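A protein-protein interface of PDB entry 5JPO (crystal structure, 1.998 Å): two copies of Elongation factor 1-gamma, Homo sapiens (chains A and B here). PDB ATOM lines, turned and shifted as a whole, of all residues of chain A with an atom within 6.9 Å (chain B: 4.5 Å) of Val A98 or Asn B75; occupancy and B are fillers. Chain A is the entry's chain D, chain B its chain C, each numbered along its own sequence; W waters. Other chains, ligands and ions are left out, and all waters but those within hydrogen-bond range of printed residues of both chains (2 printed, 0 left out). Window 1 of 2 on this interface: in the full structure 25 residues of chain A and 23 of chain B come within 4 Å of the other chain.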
ATOM      1  N   TYR A  79     -22.957  22.590 -21.640  1.00  0.00           N
ATOM      2  CA  TYR A  79     -23.187  23.682 -20.704  1.00  0.00           C
ATOM      3  C   TYR A  79     -22.752  24.998 -21.339  1.00  0.00           C
ATOM      4  O   TYR A  79     -23.461  26.006 -21.278  1.00  0.00           O
ATOM      5  CB  TYR A  79     -22.443  23.465 -19.383  1.00  0.00           C
ATOM      6  CG  TYR A  79     -22.665  24.600 -18.400  1.00  0.00           C
ATOM      7  CD1 TYR A  79     -23.667  24.526 -17.441  1.00  0.00           C
ATOM      8  CD2 TYR A  79     -21.877  25.747 -18.436  1.00  0.00           C
ATOM      9  CE1 TYR A  79     -23.887  25.562 -16.546  1.00  0.00           C
ATOM     10  CE2 TYR A  79     -22.091  26.794 -17.549  1.00  0.00           C
ATOM     11  CZ  TYR A  79     -23.097  26.691 -16.601  1.00  0.00           C
ATOM     12  OH  TYR A  79     -23.307  27.724 -15.707  1.00  0.00           O
ATOM     13  N   ARG A  87     -29.445  26.259 -18.866  1.00  0.00           N
ATOM     14  CA  ARG A  87     -28.594  25.956 -17.720  1.00  0.00           C
ATOM     15  C   ARG A  87     -29.372  25.921 -16.410  1.00  0.00           C
ATOM     16  O   ARG A  87     -28.959  25.253 -15.453  1.00  0.00           O
ATOM     17  CB  ARG A  87     -27.471  26.993 -17.594  1.00  0.00           C
ATOM     18  CG  ARG A  87     -26.378  26.874 -18.624  1.00  0.00           C
ATOM     19  CD  ARG A  87     -25.528  28.132 -18.609  1.00  0.00           C
ATOM     20  NE  ARG A  87     -24.526  28.113 -19.669  1.00  0.00           N
ATOM     21  CZ  ARG A  87     -23.974  29.201 -20.191  1.00  0.00           C
ATOM     22  NH1 ARG A  87     -24.350  30.405 -19.766  1.00  0.00           N
ATOM     23  NH2 ARG A  87     -23.059  29.086 -21.143  1.00  0.00           N
ATOM     24  N   ALA A  93     -33.253  25.853 -10.151  1.00  0.00           N
ATOM     25  CA  ALA A  93     -33.376  25.234 -11.474  1.00  0.00           C
ATOM     26  C   ALA A  93     -32.031  24.688 -11.950  1.00  0.00           C
ATOM     27  O   ALA A  93     -31.954  23.579 -12.501  1.00  0.00           O
ATOM     28  CB  ALA A  93     -33.936  26.226 -12.483  1.00  0.00           C
ATOM     29  N   ALA A  94     -30.974  25.467 -11.723  1.00  0.00           N
ATOM     30  CA  ALA A  94     -29.623  25.061 -12.090  1.00  0.00           C
ATOM     31  C   ALA A  94     -29.217  23.782 -11.368  1.00  0.00           C
ATOM     32  O   ALA A  94     -28.627  22.881 -11.967  1.00  0.00           O
ATOM     33  CB  ALA A  94     -28.624  26.188 -11.787  1.00  0.00           C
ATOM     34  N   ALA A  95     -29.513  23.700 -10.072  1.00  0.00           N
ATOM     35  CA  ALA A  95     -29.213  22.488  -9.321  1.00  0.00           C
ATOM     36  C   ALA A  95     -30.001  21.286  -9.843  1.00  0.00           C
ATOM     37  O   ALA A  95     -29.480  20.180  -9.888  1.00  0.00           O
ATOM     38  CB  ALA A  95     -29.491  22.690  -7.823  1.00  0.00           C
ATOM     39  N   GLN A  96     -31.260  21.495 -10.208  1.00  0.00           N
ATOM     40  CA  GLN A  96     -32.062  20.403 -10.736  1.00  0.00           C
ATOM     41  C   GLN A  96     -31.497  19.924 -12.073  1.00  0.00           C
ATOM     42  O   GLN A  96     -31.557  18.740 -12.411  1.00  0.00           O
ATOM     43  CB  GLN A  96     -33.508  20.836 -10.900  1.00  0.00           C
ATOM     44  CG  GLN A  96     -34.225  21.060  -9.593  1.00  0.00           C
ATOM     45  CD  GLN A  96     -35.652  21.500  -9.815  1.00  0.00           C
ATOM     46  OE1 GLN A  96     -36.562  20.677  -9.843  1.00  0.00           O
ATOM     47  NE2 GLN A  96     -35.855  22.794 -10.001  1.00  0.00           N
ATOM     48  N   VAL A  97     -30.955  20.855 -12.840  1.00  0.00           N
ATOM     49  CA  VAL A  97     -30.332  20.474 -14.085  1.00  0.00           C
ATOM     50  C   VAL A  97     -29.100  19.621 -13.819  1.00  0.00           C
ATOM     51  O   VAL A  97     -28.930  18.590 -14.469  1.00  0.00           O
ATOM     52  CB  VAL A  97     -29.983  21.707 -14.948  1.00  0.00           C
ATOM     53  CG1 VAL A  97     -28.969  21.335 -16.051  1.00  0.00           C
ATOM     54  CG2 VAL A  97     -31.262  22.259 -15.557  1.00  0.00           C
ATOM     55  N   VAL A  98     -28.272  19.992 -12.841  1.00  0.00           N
ATOM     56  CA  VAL A  98     -27.081  19.193 -12.548  1.00  0.00           C
ATOM     57  C   VAL A  98     -27.490  17.795 -12.067  1.00  0.00           C
ATOM     58  O   VAL A  98     -26.847  16.796 -12.375  1.00  0.00           O
ATOM     59  CB  VAL A  98     -26.168  19.871 -11.481  1.00  0.00           C
ATOM     60  CG1 VAL A  98     -25.083  18.902 -11.021  1.00  0.00           C
ATOM     61  CG2 VAL A  98     -25.537  21.143 -12.052  1.00  0.00           C
ATOM     62  N   GLN A  99     -28.586  17.742 -11.324  1.00  0.00           N
ATOM     63  CA  GLN A  99     -29.142  16.487 -10.822  1.00  0.00           C
ATOM     64  C   GLN A  99     -29.485  15.461 -11.920  1.00  0.00           C
ATOM     65  O   GLN A  99     -29.070  14.301 -11.848  1.00  0.00           O
ATOM     66  CB  GLN A  99     -30.388  16.806 -10.004  1.00  0.00           C
ATOM     67  CG  GLN A  99     -31.284  15.631  -9.706  1.00  0.00           C
ATOM     68  CD  GLN A  99     -32.560  16.074  -9.023  1.00  0.00           C
ATOM     69  OE1 GLN A  99     -32.552  16.427  -7.841  1.00  0.00           O
ATOM     70  NE2 GLN A  99     -33.659  16.072  -9.766  1.00  0.00           N
ATOM     71  N   TRP A 100     -30.235  15.885 -12.930  1.00  0.00           N
ATOM     72  CA  TRP A 100     -30.644  14.970 -14.003  1.00  0.00           C
ATOM     73  C   TRP A 100     -29.482  14.624 -14.926  1.00  0.00           C
ATOM     74  O   TRP A 100     -29.409  13.517 -15.479  1.00  0.00           O
ATOM     75  CB  TRP A 100     -31.810  15.564 -14.810  1.00  0.00           C
ATOM     76  CG  TRP A 100     -33.088  15.581 -14.000  1.00  0.00           C
ATOM     77  CD1 TRP A 100     -33.733  16.672 -13.483  1.00  0.00           C
ATOM     78  CD2 TRP A 100     -33.840  14.435 -13.586  1.00  0.00           C
ATOM     79  NE1 TRP A 100     -34.859  16.271 -12.782  1.00  0.00           N
ATOM     80  CE2 TRP A 100     -34.940  14.898 -12.828  1.00  0.00           C
ATOM     81  CE3 TRP A 100     -33.689  13.054 -13.771  1.00  0.00           C
ATOM     82  CZ2 TRP A 100     -35.874  14.038 -12.255  1.00  0.00           C
ATOM     83  CZ3 TRP A 100     -34.622  12.195 -13.202  1.00  0.00           C
ATOM     84  CH2 TRP A 100     -35.703  12.693 -12.458  1.00  0.00           C
ATOM     85  N   VAL A 101     -28.583  15.583 -15.110  1.00  0.00           N
ATOM     86  CA  VAL A 101     -27.377  15.351 -15.901  1.00  0.00           C
ATOM     87  C   VAL A 101     -26.527  14.283 -15.232  1.00  0.00           C
ATOM     88  O   VAL A 101     -26.038  13.350 -15.869  1.00  0.00           O
ATOM     89  CB  VAL A 101     -26.543  16.655 -16.048  1.00  0.00           C
ATOM     90  CG1 VAL A 101     -25.110  16.360 -16.517  1.00  0.00           C
ATOM     91  CG2 VAL A 101     -27.255  17.647 -16.954  1.00  0.00           C
ATOM     92  N   SER A 102     -26.331  14.443 -13.930  1.00  0.00           N
ATOM     93  CA  SER A 102     -25.551  13.481 -13.159  1.00  0.00           C
ATOM     94  C   SER A 102     -26.248  12.115 -13.104  1.00  0.00           C
ATOM     95  O   SER A 102     -25.607  11.067 -13.238  1.00  0.00           O
ATOM     96  CB  SER A 102     -25.316  14.033 -11.749  1.00  0.00           C
ATOM     97  OG  SER A 102     -24.817  13.023 -10.897  1.00  0.00           O
ATOM     98  N   PHE A 103     -27.569  12.131 -12.931  1.00  0.00           N
ATOM     99  CA  PHE A 103     -28.351  10.891 -12.889  1.00  0.00           C
ATOM    100  C   PHE A 103     -28.226  10.139 -14.221  1.00  0.00           C
ATOM    101  O   PHE A 103     -27.971   8.925 -14.242  1.00  0.00           O
ATOM    102  CB  PHE A 103     -29.821  11.189 -12.558  1.00  0.00           C
ATOM    103  CG  PHE A 103     -30.691   9.969 -12.538  1.00  0.00           C
ATOM    104  CD1 PHE A 103     -30.652   9.092 -11.465  1.00  0.00           C
ATOM    105  CD2 PHE A 103     -31.536   9.687 -13.601  1.00  0.00           C
ATOM    106  CE1 PHE A 103     -31.440   7.957 -11.446  1.00  0.00           C
ATOM    107  CE2 PHE A 103     -32.335   8.551 -13.586  1.00  0.00           C
ATOM    108  CZ  PHE A 103     -32.276   7.682 -12.501  1.00  0.00           C
ATOM    109  N   ALA A 104     -28.368  10.874 -15.324  1.00  0.00           N
ATOM    110  CA  ALA A 104     -28.143  10.322 -16.665  1.00  0.00           C
ATOM    111  C   ALA A 104     -26.804   9.598 -16.793  1.00  0.00           C
ATOM    112  O   ALA A 104     -26.749   8.442 -17.213  1.00  0.00           O
ATOM    113  CB  ALA A 104     -28.227  11.430 -17.709  1.00  0.00           C
ATOM    114  N   VAL A 155     -37.403  20.015 -15.654  1.00  0.00           N
ATOM    115  CA  VAL A 155     -37.131  21.176 -14.801  1.00  0.00           C
ATOM    116  C   VAL A 155     -37.881  22.392 -15.315  1.00  0.00           C
ATOM    117  O   VAL A 155     -37.773  22.741 -16.494  1.00  0.00           O
ATOM    118  CB  VAL A 155     -35.626  21.528 -14.739  1.00  0.00           C
ATOM    119  CG1 VAL A 155     -35.389  22.697 -13.751  1.00  0.00           C
ATOM    120  CG2 VAL A 155     -34.776  20.304 -14.365  1.00  0.00           C
ATOM    121  N   ALA A 162     -31.407  19.428 -18.758  1.00  0.00           N
ATOM    122  CA  ALA A 162     -31.918  18.178 -18.191  1.00  0.00           C
ATOM    123  C   ALA A 162     -32.576  17.307 -19.258  1.00  0.00           C
ATOM    124  O   ALA A 162     -32.224  16.145 -19.417  1.00  0.00           O
ATOM    125  CB  ALA A 162     -32.907  18.470 -17.075  1.00  0.00           C
ATOM    126  N   LYS B  19     -18.166  16.561  -0.523  1.00  0.00           N
ATOM    127  CA  LYS B  19     -18.132  17.618  -1.528  1.00  0.00           C
ATOM    128  C   LYS B  19     -19.055  18.762  -1.168  1.00  0.00           C
ATOM    129  O   LYS B  19     -18.676  19.931  -1.261  1.00  0.00           O
ATOM    130  CB  LYS B  19     -18.506  17.062  -2.903  1.00  0.00           C
ATOM    131  CG  LYS B  19     -17.521  16.036  -3.446  1.00  0.00           C
ATOM    132  CD  LYS B  19     -17.866  15.633  -4.888  1.00  0.00           C
ATOM    133  CE  LYS B  19     -19.325  15.192  -5.038  1.00  0.00           C
ATOM    134  NZ  LYS B  19     -19.571  14.444  -6.306  1.00  0.00           N
ATOM    135  N   GLU B  73     -28.264  13.562  -6.053  1.00  0.00           N
ATOM    136  CA  GLU B  73     -26.964  13.523  -6.748  1.00  0.00           C
ATOM    137  C   GLU B  73     -25.984  14.439  -6.014  1.00  0.00           C
ATOM    138  O   GLU B  73     -26.260  15.613  -5.822  1.00  0.00           O
ATOM    139  CB  GLU B  73     -27.061  13.930  -8.231  1.00  0.00           C
ATOM    140  CG  GLU B  73     -27.897  12.997  -9.107  1.00  0.00           C
ATOM    141  CD  GLU B  73     -27.287  11.607  -9.209  1.00  0.00           C
ATOM    142  OE1 GLU B  73     -26.036  11.490  -9.238  1.00  0.00           O
ATOM    143  OE2 GLU B  73     -28.057  10.627  -9.245  1.00  0.00           O
ATOM    144  N   SER B  74     -24.846  13.891  -5.607  1.00  0.00           N
ATOM    145  CA  SER B  74     -23.870  14.657  -4.842  1.00  0.00           C
ATOM    146  C   SER B  74     -23.401  15.898  -5.611  1.00  0.00           C
ATOM    147  O   SER B  74     -23.154  16.938  -5.006  1.00  0.00           O
ATOM    148  CB  SER B  74     -22.679  13.777  -4.434  1.00  0.00           C
ATOM    149  OG  SER B  74     -22.028  13.177  -5.544  1.00  0.00           O
ATOM    150  N   ASN B  75     -23.302  15.814  -6.936  1.00  0.00           N
ATOM    151  CA  ASN B  75     -22.919  16.999  -7.718  1.00  0.00           C
ATOM    152  C   ASN B  75     -23.934  18.126  -7.639  1.00  0.00           C
ATOM    153  O   ASN B  75     -23.572  19.304  -7.562  1.00  0.00           O
ATOM    154  CB  ASN B  75     -22.697  16.627  -9.190  1.00  0.00           C
ATOM    155  CG  ASN B  75     -21.505  15.723  -9.377  1.00  0.00           C
ATOM    156  OD1 ASN B  75     -20.614  15.675  -8.526  1.00  0.00           O
ATOM    157  ND2 ASN B  75     -21.481  14.994 -10.480  1.00  0.00           N
ATOM    158  N   ALA B  76     -25.212  17.779  -7.664  1.00  0.00           N
ATOM    159  CA  ALA B  76     -26.247  18.805  -7.651  1.00  0.00           C
ATOM    160  C   ALA B  76     -26.364  19.427  -6.262  1.00  0.00           C
ATOM    161  O   ALA B  76     -26.591  20.622  -6.131  1.00  0.00           O
ATOM    162  CB  ALA B  76     -27.563  18.230  -8.088  1.00  0.00           C
ATOM    163  N   ILE B  77     -26.224  18.603  -5.232  1.00  0.00           N
ATOM    164  CA  ILE B  77     -26.280  19.095  -3.857  1.00  0.00           C
ATOM    165  C   ILE B  77     -25.126  20.052  -3.584  1.00  0.00           C
ATOM    166  O   ILE B  77     -25.317  21.131  -3.016  1.00  0.00           O
ATOM    167  CB  ILE B  77     -26.234  17.942  -2.842  1.00  0.00           C
ATOM    168  CG1 ILE B  77     -27.482  17.068  -3.000  1.00  0.00           C
ATOM    169  CG2 ILE B  77     -26.142  18.490  -1.419  1.00  0.00           C
ATOM    170  CD1 ILE B  77     -27.428  15.765  -2.230  1.00  0.00           C
ATOM    171  N   ALA B  78     -23.927  19.651  -3.998  1.00  0.00           N
ATOM    172  CA  ALA B  78     -22.755  20.497  -3.821  1.00  0.00           C
ATOM    173  C   ALA B  78     -22.957  21.791  -4.591  1.00  0.00           C
ATOM    174  O   ALA B  78     -22.646  22.872  -4.093  1.00  0.00           O
ATOM    175  CB  ALA B  78     -21.483  19.774  -4.281  1.00  0.00           C
ATOM    176  N   TYR B  79     -23.502  21.688  -5.799  1.00  0.00           N
ATOM    177  CA  TYR B  79     -23.766  22.880  -6.592  1.00  0.00           C
ATOM    178  C   TYR B  79     -24.705  23.809  -5.816  1.00  0.00           C
ATOM    179  O   TYR B  79     -24.468  25.018  -5.715  1.00  0.00           O
ATOM    180  CB  TYR B  79     -24.372  22.527  -7.968  1.00  0.00           C
ATOM    181  CG  TYR B  79     -24.666  23.756  -8.815  1.00  0.00           C
ATOM    182  CD1 TYR B  79     -23.778  24.178  -9.800  1.00  0.00           C
ATOM    183  CD2 TYR B  79     -25.818  24.508  -8.610  1.00  0.00           C
ATOM    184  CE1 TYR B  79     -24.035  25.316 -10.562  1.00  0.00           C
ATOM    185  CE2 TYR B  79     -26.082  25.652  -9.363  1.00  0.00           C
ATOM    186  CZ  TYR B  79     -25.188  26.048 -10.336  1.00  0.00           C
ATOM    187  OH  TYR B  79     -25.460  27.178 -11.081  1.00  0.00           O
ATOM    188  N   VAL B 101     -15.634  18.100 -12.918  1.00  0.00           N
ATOM    189  CA  VAL B 101     -16.583  17.274 -12.174  1.00  0.00           C
ATOM    190  C   VAL B 101     -16.945  16.040 -12.989  1.00  0.00           C
ATOM    191  O   VAL B 101     -16.907  14.912 -12.478  1.00  0.00           O
ATOM    192  CB  VAL B 101     -17.843  18.076 -11.810  1.00  0.00           C
ATOM    193  CG1 VAL B 101     -18.964  17.154 -11.347  1.00  0.00           C
ATOM    194  CG2 VAL B 101     -17.500  19.130 -10.730  1.00  0.00           C
ATOM    195  N   ASP B 105     -16.077  11.959 -12.269  1.00  0.00           N
ATOM    196  CA  ASP B 105     -17.075  10.889 -12.295  1.00  0.00           C
ATOM    197  C   ASP B 105     -16.751   9.821 -13.336  1.00  0.00           C
ATOM    198  O   ASP B 105     -16.788   8.629 -13.045  1.00  0.00           O
ATOM    199  CB  ASP B 105     -18.471  11.448 -12.577  1.00  0.00           C
ATOM    200  CG  ASP B 105     -19.030  12.255 -11.415  1.00  0.00           C
ATOM    201  OD1 ASP B 105     -18.658  11.981 -10.249  1.00  0.00           O
ATOM    202  OD2 ASP B 105     -19.847  13.168 -11.678  1.00  0.00           O
HETATM  203  O   HOH W   1     -22.458  11.426 -12.481  1.00  0.00           O
HETATM  204  O   HOH W   2     -23.538  13.472  -8.544  1.00  0.00           O
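OE1 of Glu B73 is in hydrogen-bond range of OG of Ser A102 (2.6 Å).
The side-chain amino group (NZ) of Lys B19 lies within hydrogen-bond range of the side-chain amide oxygen (OD1) of Asn B75. The side-chain amide nitrogen (ND2) of Asn B75 is in hydrogen-bond range of the side-chain carboxylate (OD2) of Asp B105 (2.7 Å). The indole nitrogen (NE1) of Trp A100 lies close to the side-chain amide nitrogen (NE2) of Gln A99 (3.3 Å).
Among the printed residues, merely in contact across the chains: Ala A94 with Tyr B79 (3.4 Å), Ala A95 with Ala B76 (3.3 Å), Val A98 with Asn B75 (3.7 Å), Val A98 with Ala B76 (3.5 Å), Gln A99 with Glu B73 (3.3 Å), Gln A99 with Ala B76 (3.4 Å), Ser A102 with Asn B75 (3.9 Å) and Phe A103 with Glu B73 (3.7 Å).
Of the printed residues of chain B, Ala A94 touches Tyr B79. Of the printed residues of chain B, Val A98 touches Asn B75 and Ala B76. Trp A100 touches none of the printed residues of chain B. Of the printed residues of chain B, Ser A102 touches Glu B73 (2.6 Å) and Asn B75 (3.9 Å). Of the printed residues of chain B, Phe A103 touches Glu B73. Lys B19 touches none of the printed residues of chain A. Printed residues of chain A within 4 Å of Glu B73: Gln A99 (3.3 Å), Ser A102 (2.6 Å) and Phe A103 (3.7 Å). Printed residues of chain A within 4 Å of Ala B76: Ala A95 (3.3 Å), Val A98 (3.5 Å) and Gln A99 (3.4 Å). The nearest residue of chain B that does not touch Val A98 is Tyr B79 (4.2 Å). The nearest residue of chain A that does not touch Asn B75 is Gln A99 (5.9 Å).
Of the 10 printed residues of chain B, 4 touch a printed residue of chain A. Printed residues of chain B that touch a printed residue of chain A: Glu B73, Asn B75, Ala B76 and Tyr B79. Hydrophobic or aromatic side chains of chain B within 4 Å of the printed part of chain A: Ala B76 and Tyr B79. Of the 16 printed residues of chain A, 6 touch a printed residue of chain B. Printed residues of chain A that touch a printed residue of chain B: Ala A94, Ala A95, Val A98, Gln A99, Ser A102 and Phe A103. Hydrophobic or aromatic side chains of chain A within 4 Å of the printed part of chain B: Ala A94, Ala A95, Val A98 and Phe A103. Among the printed residues, 9 pairs touch across the chains.
Positions printed for both chains: 79 and 101.
Water W2 lies within hydrogen-bond range of OG of Ser A102 (2.7 Å), N of Asn B75 (2.9 Å), N of Ser B74 (3.2 Å) and OE1 of Glu B73 (3.3 Å). Water W1 lies within hydrogen-bond range of OD2 of Asp B105 (3.2 Å) and O of Ser A102 (3.3 Å).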
